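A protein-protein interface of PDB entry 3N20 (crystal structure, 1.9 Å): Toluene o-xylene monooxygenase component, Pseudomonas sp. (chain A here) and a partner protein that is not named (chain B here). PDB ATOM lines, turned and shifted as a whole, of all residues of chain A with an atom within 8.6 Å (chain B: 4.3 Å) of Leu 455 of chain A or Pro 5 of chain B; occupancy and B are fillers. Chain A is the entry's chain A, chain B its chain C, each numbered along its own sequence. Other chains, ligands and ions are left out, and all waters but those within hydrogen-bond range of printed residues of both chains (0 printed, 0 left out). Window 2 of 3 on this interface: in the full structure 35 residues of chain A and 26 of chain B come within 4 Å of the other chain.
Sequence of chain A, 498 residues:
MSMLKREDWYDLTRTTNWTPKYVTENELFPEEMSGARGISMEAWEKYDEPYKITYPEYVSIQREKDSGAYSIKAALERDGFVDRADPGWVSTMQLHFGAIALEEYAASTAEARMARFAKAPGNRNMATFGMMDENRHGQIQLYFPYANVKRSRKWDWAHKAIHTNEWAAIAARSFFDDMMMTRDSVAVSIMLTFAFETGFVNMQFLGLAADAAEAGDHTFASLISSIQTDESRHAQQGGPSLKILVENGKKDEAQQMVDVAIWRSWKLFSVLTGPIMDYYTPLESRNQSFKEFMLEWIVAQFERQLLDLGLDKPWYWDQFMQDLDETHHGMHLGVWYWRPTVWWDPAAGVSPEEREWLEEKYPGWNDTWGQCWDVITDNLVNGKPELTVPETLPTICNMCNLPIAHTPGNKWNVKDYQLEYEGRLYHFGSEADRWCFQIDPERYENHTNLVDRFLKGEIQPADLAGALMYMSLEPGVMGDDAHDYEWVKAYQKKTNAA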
ATOM      1  N   THR A 392       7.919 -16.450 -16.540  1.00  0.00           N
ATOM      2  CA  THR A 392       7.599 -17.553 -15.646  1.00  0.00           C
ATOM      3  C   THR A 392       8.523 -17.523 -14.436  1.00  0.00           C
ATOM      4  O   THR A 392       9.421 -16.691 -14.361  1.00  0.00           O
ATOM      5  CB  THR A 392       7.737 -18.918 -16.344  1.00  0.00           C
ATOM      6  OG1 THR A 392       7.223 -19.934 -15.475  1.00  0.00           O
ATOM      7  CG2 THR A 392       9.195 -19.214 -16.674  1.00  0.00           C
ATOM      8  N   LEU A 393       8.298 -18.422 -13.484  1.00  0.00           N
ATOM      9  CA  LEU A 393       9.143 -18.476 -12.302  1.00  0.00           C
ATOM     10  C   LEU A 393      10.156 -19.596 -12.479  1.00  0.00           C
ATOM     11  O   LEU A 393       9.895 -20.584 -13.164  1.00  0.00           O
ATOM     12  CB  LEU A 393       8.346 -18.791 -11.026  1.00  0.00           C
ATOM     13  CG  LEU A 393       6.903 -18.398 -10.692  1.00  0.00           C
ATOM     14  CD1 LEU A 393       6.854 -18.143  -9.185  1.00  0.00           C
ATOM     15  CD2 LEU A 393       6.436 -17.163 -11.444  1.00  0.00           C
ATOM     16  N   THR A 395      12.569 -22.746 -11.046  1.00  0.00           N
ATOM     17  CA  THR A 395      12.334 -23.757 -10.026  1.00  0.00           C
ATOM     18  C   THR A 395      13.142 -23.343  -8.792  1.00  0.00           C
ATOM     19  O   THR A 395      14.309 -22.959  -8.904  1.00  0.00           O
ATOM     20  CB  THR A 395      12.786 -25.140 -10.509  1.00  0.00           C
ATOM     21  OG1 THR A 395      12.119 -25.438 -11.739  1.00  0.00           O
ATOM     22  CG2 THR A 395      12.430 -26.211  -9.488  1.00  0.00           C
ATOM     23  N   LEU A 425       6.266 -33.881  -3.903  1.00  0.00           N
ATOM     24  CA  LEU A 425       7.530 -33.860  -4.622  1.00  0.00           C
ATOM     25  C   LEU A 425       8.295 -32.583  -4.273  1.00  0.00           C
ATOM     26  O   LEU A 425       7.815 -31.471  -4.501  1.00  0.00           O
ATOM     27  CB  LEU A 425       7.286 -33.915  -6.130  1.00  0.00           C
ATOM     28  CG  LEU A 425       8.549 -34.010  -6.987  1.00  0.00           C
ATOM     29  CD1 LEU A 425       9.320 -35.274  -6.600  1.00  0.00           C
ATOM     30  CD2 LEU A 425       8.172 -34.030  -8.471  1.00  0.00           C
ATOM     31  N   HIS A 427      11.933 -30.299  -4.558  1.00  0.00           N
ATOM     32  CA  HIS A 427      13.036 -30.043  -5.475  1.00  0.00           C
ATOM     33  C   HIS A 427      14.184 -29.413  -4.707  1.00  0.00           C
ATOM     34  O   HIS A 427      13.972 -28.546  -3.854  1.00  0.00           O
ATOM     35  CB  HIS A 427      12.603 -29.112  -6.607  1.00  0.00           C
ATOM     36  CG  HIS A 427      11.552 -29.700  -7.491  1.00  0.00           C
ATOM     37  ND1 HIS A 427      10.211 -29.649  -7.181  1.00  0.00           N
ATOM     38  CD2 HIS A 427      11.648 -30.414  -8.637  1.00  0.00           C
ATOM     39  CE1 HIS A 427       9.528 -30.309  -8.099  1.00  0.00           C
ATOM     40  NE2 HIS A 427      10.376 -30.784  -8.993  1.00  0.00           N
ATOM     41  N   ASN A 449       7.835 -23.048  -0.592  1.00  0.00           N
ATOM     42  CA  ASN A 449       8.615 -22.000  -1.226  1.00  0.00           C
ATOM     43  C   ASN A 449       7.661 -21.210  -2.112  1.00  0.00           C
ATOM     44  O   ASN A 449       6.491 -21.568  -2.249  1.00  0.00           O
ATOM     45  CB  ASN A 449       9.792 -22.555  -2.046  1.00  0.00           C
ATOM     46  CG  ASN A 449       9.357 -23.340  -3.275  1.00  0.00           C
ATOM     47  OD1 ASN A 449       8.388 -22.995  -3.952  1.00  0.00           O
ATOM     48  ND2 ASN A 449      10.106 -24.393  -3.585  1.00  0.00           N
ATOM     49  N   LEU A 450       8.163 -20.134  -2.703  1.00  0.00           N
ATOM     50  CA  LEU A 450       7.354 -19.264  -3.545  1.00  0.00           C
ATOM     51  C   LEU A 450       6.633 -19.995  -4.682  1.00  0.00           C
ATOM     52  O   LEU A 450       5.474 -19.693  -4.988  1.00  0.00           O
ATOM     53  CB  LEU A 450       8.237 -18.147  -4.100  1.00  0.00           C
ATOM     54  CG  LEU A 450       7.596 -16.768  -4.231  1.00  0.00           C
ATOM     55  CD1 LEU A 450       6.778 -16.450  -2.986  1.00  0.00           C
ATOM     56  CD2 LEU A 450       8.698 -15.728  -4.438  1.00  0.00           C
ATOM     57  N   VAL A 451       7.317 -20.947  -5.309  1.00  0.00           N
ATOM     58  CA  VAL A 451       6.723 -21.714  -6.399  1.00  0.00           C
ATOM     59  C   VAL A 451       5.577 -22.572  -5.859  1.00  0.00           C
ATOM     60  O   VAL A 451       4.505 -22.653  -6.468  1.00  0.00           O
ATOM     61  CB  VAL A 451       7.776 -22.626  -7.090  1.00  0.00           C
ATOM     62  CG1 VAL A 451       7.092 -23.578  -8.068  1.00  0.00           C
ATOM     63  CG2 VAL A 451       8.794 -21.773  -7.830  1.00  0.00           C
ATOM     64  N   ASP A 452       5.807 -23.214  -4.715  1.00  0.00           N
ATOM     65  CA  ASP A 452       4.784 -24.045  -4.095  1.00  0.00           C
ATOM     66  C   ASP A 452       3.527 -23.217  -3.842  1.00  0.00           C
ATOM     67  O   ASP A 452       2.414 -23.666  -4.102  1.00  0.00           O
ATOM     68  CB  ASP A 452       5.283 -24.628  -2.768  1.00  0.00           C
ATOM     69  CG  ASP A 452       6.473 -25.554  -2.948  1.00  0.00           C
ATOM     70  OD1 ASP A 452       6.476 -26.317  -3.934  1.00  0.00           O
ATOM     71  OD2 ASP A 452       7.399 -25.532  -2.107  1.00  0.00           O
ATOM     72  N   ARG A 453       3.713 -22.007  -3.331  1.00  0.00           N
ATOM     73  CA  ARG A 453       2.591 -21.124  -3.042  1.00  0.00           C
ATOM     74  C   ARG A 453       1.869 -20.721  -4.322  1.00  0.00           C
ATOM     75  O   ARG A 453       0.639 -20.678  -4.358  1.00  0.00           O
ATOM     76  CB  ARG A 453       3.084 -19.884  -2.288  1.00  0.00           C
ATOM     77  CG  ARG A 453       3.805 -20.246  -0.999  1.00  0.00           C
ATOM     78  CD  ARG A 453       4.257 -19.035  -0.212  1.00  0.00           C
ATOM     79  NE  ARG A 453       5.243 -19.419   0.794  1.00  0.00           N
ATOM     80  CZ  ARG A 453       5.871 -18.565   1.597  1.00  0.00           C
ATOM     81  NH1 ARG A 453       5.612 -17.262   1.519  1.00  0.00           N
ATOM     82  NH2 ARG A 453       6.774 -19.013   2.460  1.00  0.00           N
ATOM     83  N   PHE A 454       2.638 -20.429  -5.366  1.00  0.00           N
ATOM     84  CA  PHE A 454       2.062 -20.042  -6.649  1.00  0.00           C
ATOM     85  C   PHE A 454       1.168 -21.178  -7.151  1.00  0.00           C
ATOM     86  O   PHE A 454       0.015 -20.958  -7.540  1.00  0.00           O
ATOM     87  CB  PHE A 454       3.171 -19.769  -7.673  1.00  0.00           C
ATOM     88  CG  PHE A 454       2.679 -19.158  -8.960  1.00  0.00           C
ATOM     89  CD1 PHE A 454       2.374 -17.801  -9.029  1.00  0.00           C
ATOM     90  CD2 PHE A 454       2.472 -19.951 -10.089  1.00  0.00           C
ATOM     91  CE1 PHE A 454       1.868 -17.238 -10.206  1.00  0.00           C
ATOM     92  CE2 PHE A 454       1.966 -19.397 -11.270  1.00  0.00           C
ATOM     93  CZ  PHE A 454       1.663 -18.037 -11.325  1.00  0.00           C
ATOM     94  N   LEU A 455       1.704 -22.395  -7.123  1.00  0.00           N
ATOM     95  CA  LEU A 455       0.979 -23.570  -7.583  1.00  0.00           C
ATOM     96  C   LEU A 455      -0.192 -23.964  -6.686  1.00  0.00           C
ATOM     97  O   LEU A 455      -1.087 -24.682  -7.120  1.00  0.00           O
ATOM     98  CB  LEU A 455       1.943 -24.756  -7.726  1.00  0.00           C
ATOM     99  CG  LEU A 455       3.026 -24.595  -8.801  1.00  0.00           C
ATOM    100  CD1 LEU A 455       3.894 -25.847  -8.868  1.00  0.00           C
ATOM    101  CD2 LEU A 455       2.370 -24.335 -10.148  1.00  0.00           C
ATOM    102  N   LYS A 456      -0.185 -23.504  -5.437  1.00  0.00           N
ATOM    103  CA  LYS A 456      -1.259 -23.818  -4.497  1.00  0.00           C
ATOM    104  C   LYS A 456      -2.440 -22.861  -4.601  1.00  0.00           C
ATOM    105  O   LYS A 456      -3.497 -23.119  -4.035  1.00  0.00           O
ATOM    106  CB  LYS A 456      -0.755 -23.760  -3.055  1.00  0.00           C
ATOM    107  CG  LYS A 456       0.188 -24.858  -2.648  1.00  0.00           C
ATOM    108  CD  LYS A 456       0.485 -24.747  -1.154  1.00  0.00           C
ATOM    109  CE  LYS A 456      -0.811 -24.799  -0.343  1.00  0.00           C
ATOM    110  NZ  LYS A 456      -0.576 -24.740   1.124  1.00  0.00           N
ATOM    111  N   GLY A 457      -2.257 -21.746  -5.294  1.00  0.00           N
ATOM    112  CA  GLY A 457      -3.336 -20.784  -5.416  1.00  0.00           C
ATOM    113  C   GLY A 457      -3.259 -19.683  -4.372  1.00  0.00           C
ATOM    114  O   GLY A 457      -4.174 -18.872  -4.251  1.00  0.00           O
ATOM    115  N   GLU A 458      -2.162 -19.644  -3.620  1.00  0.00           N
ATOM    116  CA  GLU A 458      -1.986 -18.638  -2.578  1.00  0.00           C
ATOM    117  C   GLU A 458      -1.571 -17.266  -3.104  1.00  0.00           C
ATOM    118  O   GLU A 458      -1.603 -16.276  -2.376  1.00  0.00           O
ATOM    119  CB  GLU A 458      -0.986 -19.143  -1.541  1.00  0.00           C
ATOM    120  CG  GLU A 458      -1.590 -20.203  -0.623  1.00  0.00           C
ATOM    121  CD  GLU A 458      -0.568 -20.872   0.279  1.00  0.00           C
ATOM    122  OE1 GLU A 458       0.493 -20.267   0.537  1.00  0.00           O
ATOM    123  OE2 GLU A 458      -0.843 -22.002   0.745  1.00  0.00           O
ATOM    124  N   ILE A 459      -1.181 -17.212  -4.370  1.00  0.00           N
ATOM    125  CA  ILE A 459      -0.793 -15.956  -4.994  1.00  0.00           C
ATOM    126  C   ILE A 459      -1.892 -15.627  -6.002  1.00  0.00           C
ATOM    127  O   ILE A 459      -2.093 -16.356  -6.977  1.00  0.00           O
ATOM    128  CB  ILE A 459       0.583 -16.086  -5.694  1.00  0.00           C
ATOM    129  CG1 ILE A 459       1.675 -16.309  -4.636  1.00  0.00           C
ATOM    130  CG2 ILE A 459       0.881 -14.841  -6.522  1.00  0.00           C
ATOM    131  CD1 ILE A 459       3.082 -16.435  -5.200  1.00  0.00           C
ATOM    132  N   GLN A 460      -2.614 -14.538  -5.738  1.00  0.00           N
ATOM    133  CA  GLN A 460      -3.733 -14.102  -6.579  1.00  0.00           C
ATOM    134  C   GLN A 460      -3.672 -12.600  -6.830  1.00  0.00           C
ATOM    135  O   GLN A 460      -3.473 -11.831  -5.899  1.00  0.00           O
ATOM    136  CB  GLN A 460      -5.059 -14.422  -5.880  1.00  0.00           C
ATOM    137  CG  GLN A 460      -5.337 -15.892  -5.636  1.00  0.00           C
ATOM    138  CD  GLN A 460      -5.542 -16.644  -6.923  1.00  0.00           C
ATOM    139  OE1 GLN A 460      -5.996 -16.073  -7.915  1.00  0.00           O
ATOM    140  NE2 GLN A 460      -5.224 -17.932  -6.917  1.00  0.00           N
ATOM    141  N   ALA A 462      -3.164 -15.096 -10.053  1.00  0.00           N
ATOM    142  CA  ALA A 462      -2.114 -16.079 -10.270  1.00  0.00           C
ATOM    143  C   ALA A 462      -1.297 -15.817 -11.533  1.00  0.00           C
ATOM    144  O   ALA A 462      -1.232 -16.659 -12.431  1.00  0.00           O
ATOM    145  CB  ALA A 462      -2.712 -17.479 -10.312  1.00  0.00           C
ATOM    146  N   PHE B   4      -1.298 -28.832 -16.233  1.00  0.00           N
ATOM    147  CA  PHE B   4      -0.439 -29.653 -15.380  1.00  0.00           C
ATOM    148  C   PHE B   4       0.947 -29.014 -15.293  1.00  0.00           C
ATOM    149  O   PHE B   4       1.580 -28.743 -16.314  1.00  0.00           O
ATOM    150  CB  PHE B   4      -0.337 -31.047 -16.009  1.00  0.00           C
ATOM    151  CG  PHE B   4       0.367 -32.064 -15.157  1.00  0.00           C
ATOM    152  CD1 PHE B   4      -0.297 -32.708 -14.116  1.00  0.00           C
ATOM    153  CD2 PHE B   4       1.684 -32.417 -15.433  1.00  0.00           C
ATOM    154  CE1 PHE B   4       0.341 -33.697 -13.366  1.00  0.00           C
ATOM    155  CE2 PHE B   4       2.333 -33.402 -14.690  1.00  0.00           C
ATOM    156  CZ  PHE B   4       1.660 -34.046 -13.654  1.00  0.00           C
ATOM    157  N   PRO B   5       1.442 -28.770 -14.070  1.00  0.00           N
ATOM    158  CA  PRO B   5       2.764 -28.153 -13.933  1.00  0.00           C
ATOM    159  C   PRO B   5       3.952 -29.108 -14.010  1.00  0.00           C
ATOM    160  O   PRO B   5       3.936 -30.189 -13.421  1.00  0.00           O
ATOM    161  CB  PRO B   5       2.675 -27.477 -12.570  1.00  0.00           C
ATOM    162  CG  PRO B   5       1.881 -28.488 -11.787  1.00  0.00           C
ATOM    163  CD  PRO B   5       0.767 -28.860 -12.762  1.00  0.00           C
ATOM    164  N   ILE B   6       4.979 -28.704 -14.750  1.00  0.00           N
ATOM    165  CA  ILE B   6       6.202 -29.489 -14.854  1.00  0.00           C
ATOM    166  C   ILE B   6       7.384 -28.530 -14.746  1.00  0.00           C
ATOM    167  O   ILE B   6       7.232 -27.326 -14.932  1.00  0.00           O
ATOM    168  CB  ILE B   6       6.284 -30.298 -16.194  1.00  0.00           C
ATOM    169  CG1 ILE B   6       6.191 -29.369 -17.407  1.00  0.00           C
ATOM    170  CG2 ILE B   6       5.185 -31.353 -16.230  1.00  0.00           C
ATOM    171  CD1 ILE B   6       7.533 -28.837 -17.874  1.00  0.00           C
ATOM    172  N   LEU B  18       9.545 -23.291 -14.148  1.00  0.00           N
ATOM    173  CA  LEU B  18       8.179 -23.764 -14.025  1.00  0.00           C
ATOM    174  C   LEU B  18       7.519 -23.552 -15.381  1.00  0.00           C
ATOM    175  O   LEU B  18       7.544 -22.443 -15.918  1.00  0.00           O
ATOM    176  CB  LEU B  18       7.424 -22.963 -12.960  1.00  0.00           C
ATOM    177  CG  LEU B  18       5.900 -23.155 -12.931  1.00  0.00           C
ATOM    178  CD1 LEU B  18       5.575 -24.591 -12.533  1.00  0.00           C
ATOM    179  CD2 LEU B  18       5.261 -22.172 -11.950  1.00  0.00           C
ATOM    180  N   VAL B  19       6.952 -24.616 -15.948  1.00  0.00           N
ATOM    181  CA  VAL B  19       6.271 -24.522 -17.237  1.00  0.00           C
ATOM    182  C   VAL B  19       4.965 -25.307 -17.205  1.00  0.00           C
ATOM    183  O   VAL B  19       4.970 -26.538 -17.109  1.00  0.00           O
ATOM    184  CB  VAL B  19       7.124 -25.084 -18.400  1.00  0.00           C
ATOM    185  CG1 VAL B  19       6.397 -24.853 -19.725  1.00  0.00           C
ATOM    186  CG2 VAL B  19       8.500 -24.427 -18.417  1.00  0.00           C
ATOM    187  N   PRO B  75       2.916 -34.334 -10.379  1.00  0.00           N
ATOM    188  CA  PRO B  75       2.803 -32.893 -10.613  1.00  0.00           C
ATOM    189  C   PRO B  75       4.128 -32.219 -10.301  1.00  0.00           C
ATOM    190  O   PRO B  75       4.790 -32.566  -9.315  1.00  0.00           O
ATOM    191  CB  PRO B  75       1.704 -32.465  -9.640  1.00  0.00           C
ATOM    192  CG  PRO B  75       0.846 -33.699  -9.529  1.00  0.00           C
ATOM    193  CD  PRO B  75       1.879 -34.808  -9.447  1.00  0.00           C
ATOM    194  N   THR B  76       4.536 -31.291 -11.157  1.00  0.00           N
ATOM    195  CA  THR B  76       5.760 -30.558 -10.911  1.00  0.00           C
ATOM    196  C   THR B  76       7.034 -31.376 -11.227  1.00  0.00           C
ATOM    197  O   THR B  76       8.150 -30.956 -10.940  1.00  0.00           O
ATOM    198  CB  THR B  76       5.693 -30.040  -9.440  1.00  0.00           C
ATOM    199  OG1 THR B  76       5.734 -28.608  -9.434  1.00  0.00           O
ATOM    200  CG2 THR B  76       6.771 -30.628  -8.587  1.00  0.00           C
ATOM    201  N   GLU B  77       6.844 -32.536 -11.849  1.00  0.00           N
ATOM    202  CA  GLU B  77       7.942 -33.422 -12.252  1.00  0.00           C
ATOM    203  C   GLU B  77       8.956 -32.661 -13.122  1.00  0.00           C
ATOM    204  O   GLU B  77       8.572 -31.890 -14.012  1.00  0.00           O
ATOM    205  CB  GLU B  77       7.367 -34.586 -13.065  1.00  0.00           C
ATOM    206  CG  GLU B  77       8.359 -35.647 -13.490  1.00  0.00           C
ATOM    207  CD  GLU B  77       8.468 -36.765 -12.476  1.00  0.00           C
ATOM    208  OE1 GLU B  77       7.407 -37.245 -12.015  1.00  0.00           O
ATOM    209  OE2 GLU B  77       9.608 -37.169 -12.150  1.00  0.00           O
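Among the printed residues, pairs that only touch across the chains: Leu 425 of chain A with Pro 75 of chain B (3.8 Å), Leu 425 of chain A with Thr 76 of chain B (3.7 Å), Leu 425 of chain A with Glu 77 of chain B (3.8 Å), Leu 455 of chain A with Pro 5 of chain B (3.98 Å) and Leu 455 of chain A with Thr 76 of chain B (3.4 Å).
The backbone NH of Thr 76 of chain B lies within hydrogen-bond range of the backbone carbonyl oxygen of Pro 5 of chain B (2.6 Å).
The backbone carbonyl oxygen (O) of Leu 18 of chain B is in hydrogen-bond range of the side-chain hydroxyl (OG1) of Thr 392 of chain A (2.6 Å).
The backbone carbonyl oxygen of Leu 393 of chain A lies within hydrogen-bond range of the backbone NH of Leu 18 of chain B (2.9 Å).
NE2 of His 427 of chain A lies within hydrogen-bond range of O of Thr 76 of chain B (3.0 Å).
Printed residues of chain B within 4 Å of Thr 392 of chain A: Leu 18.
Of the printed residues of chain B, Leu 393 of chain A touches Leu 18 (2.9 Å).
Of the printed residues of chain B, Leu 455 of chain A touches Pro 5 (3.98 Å) and Thr 76 (3.4 Å).
Of the printed residues of chain A, Pro 5 of chain B touches Leu 455 (3.98 Å).
Of the printed residues of chain A, Pro 75 of chain B touches Leu 425 (3.8 Å).
Of the printed residues of chain A, Glu 77 of chain B touches Leu 425.
The nearest residue of chain A that does not touch Pro 5 of chain B is Val 451 of chain A (7.4 Å).
Hydrophobic or aromatic side chains of chain B within 4 Å of the printed part of chain A: Pro 5 and Leu 18.
Hydrophobic or aromatic side chains of chain A within 4 Å of the printed part of chain B: Leu 425, His 427 and Leu 455.
Among the printed residues, no Asp or Glu carboxylate lies within 4 Å of a Lys or Arg side-chain nitrogen of the other chain.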
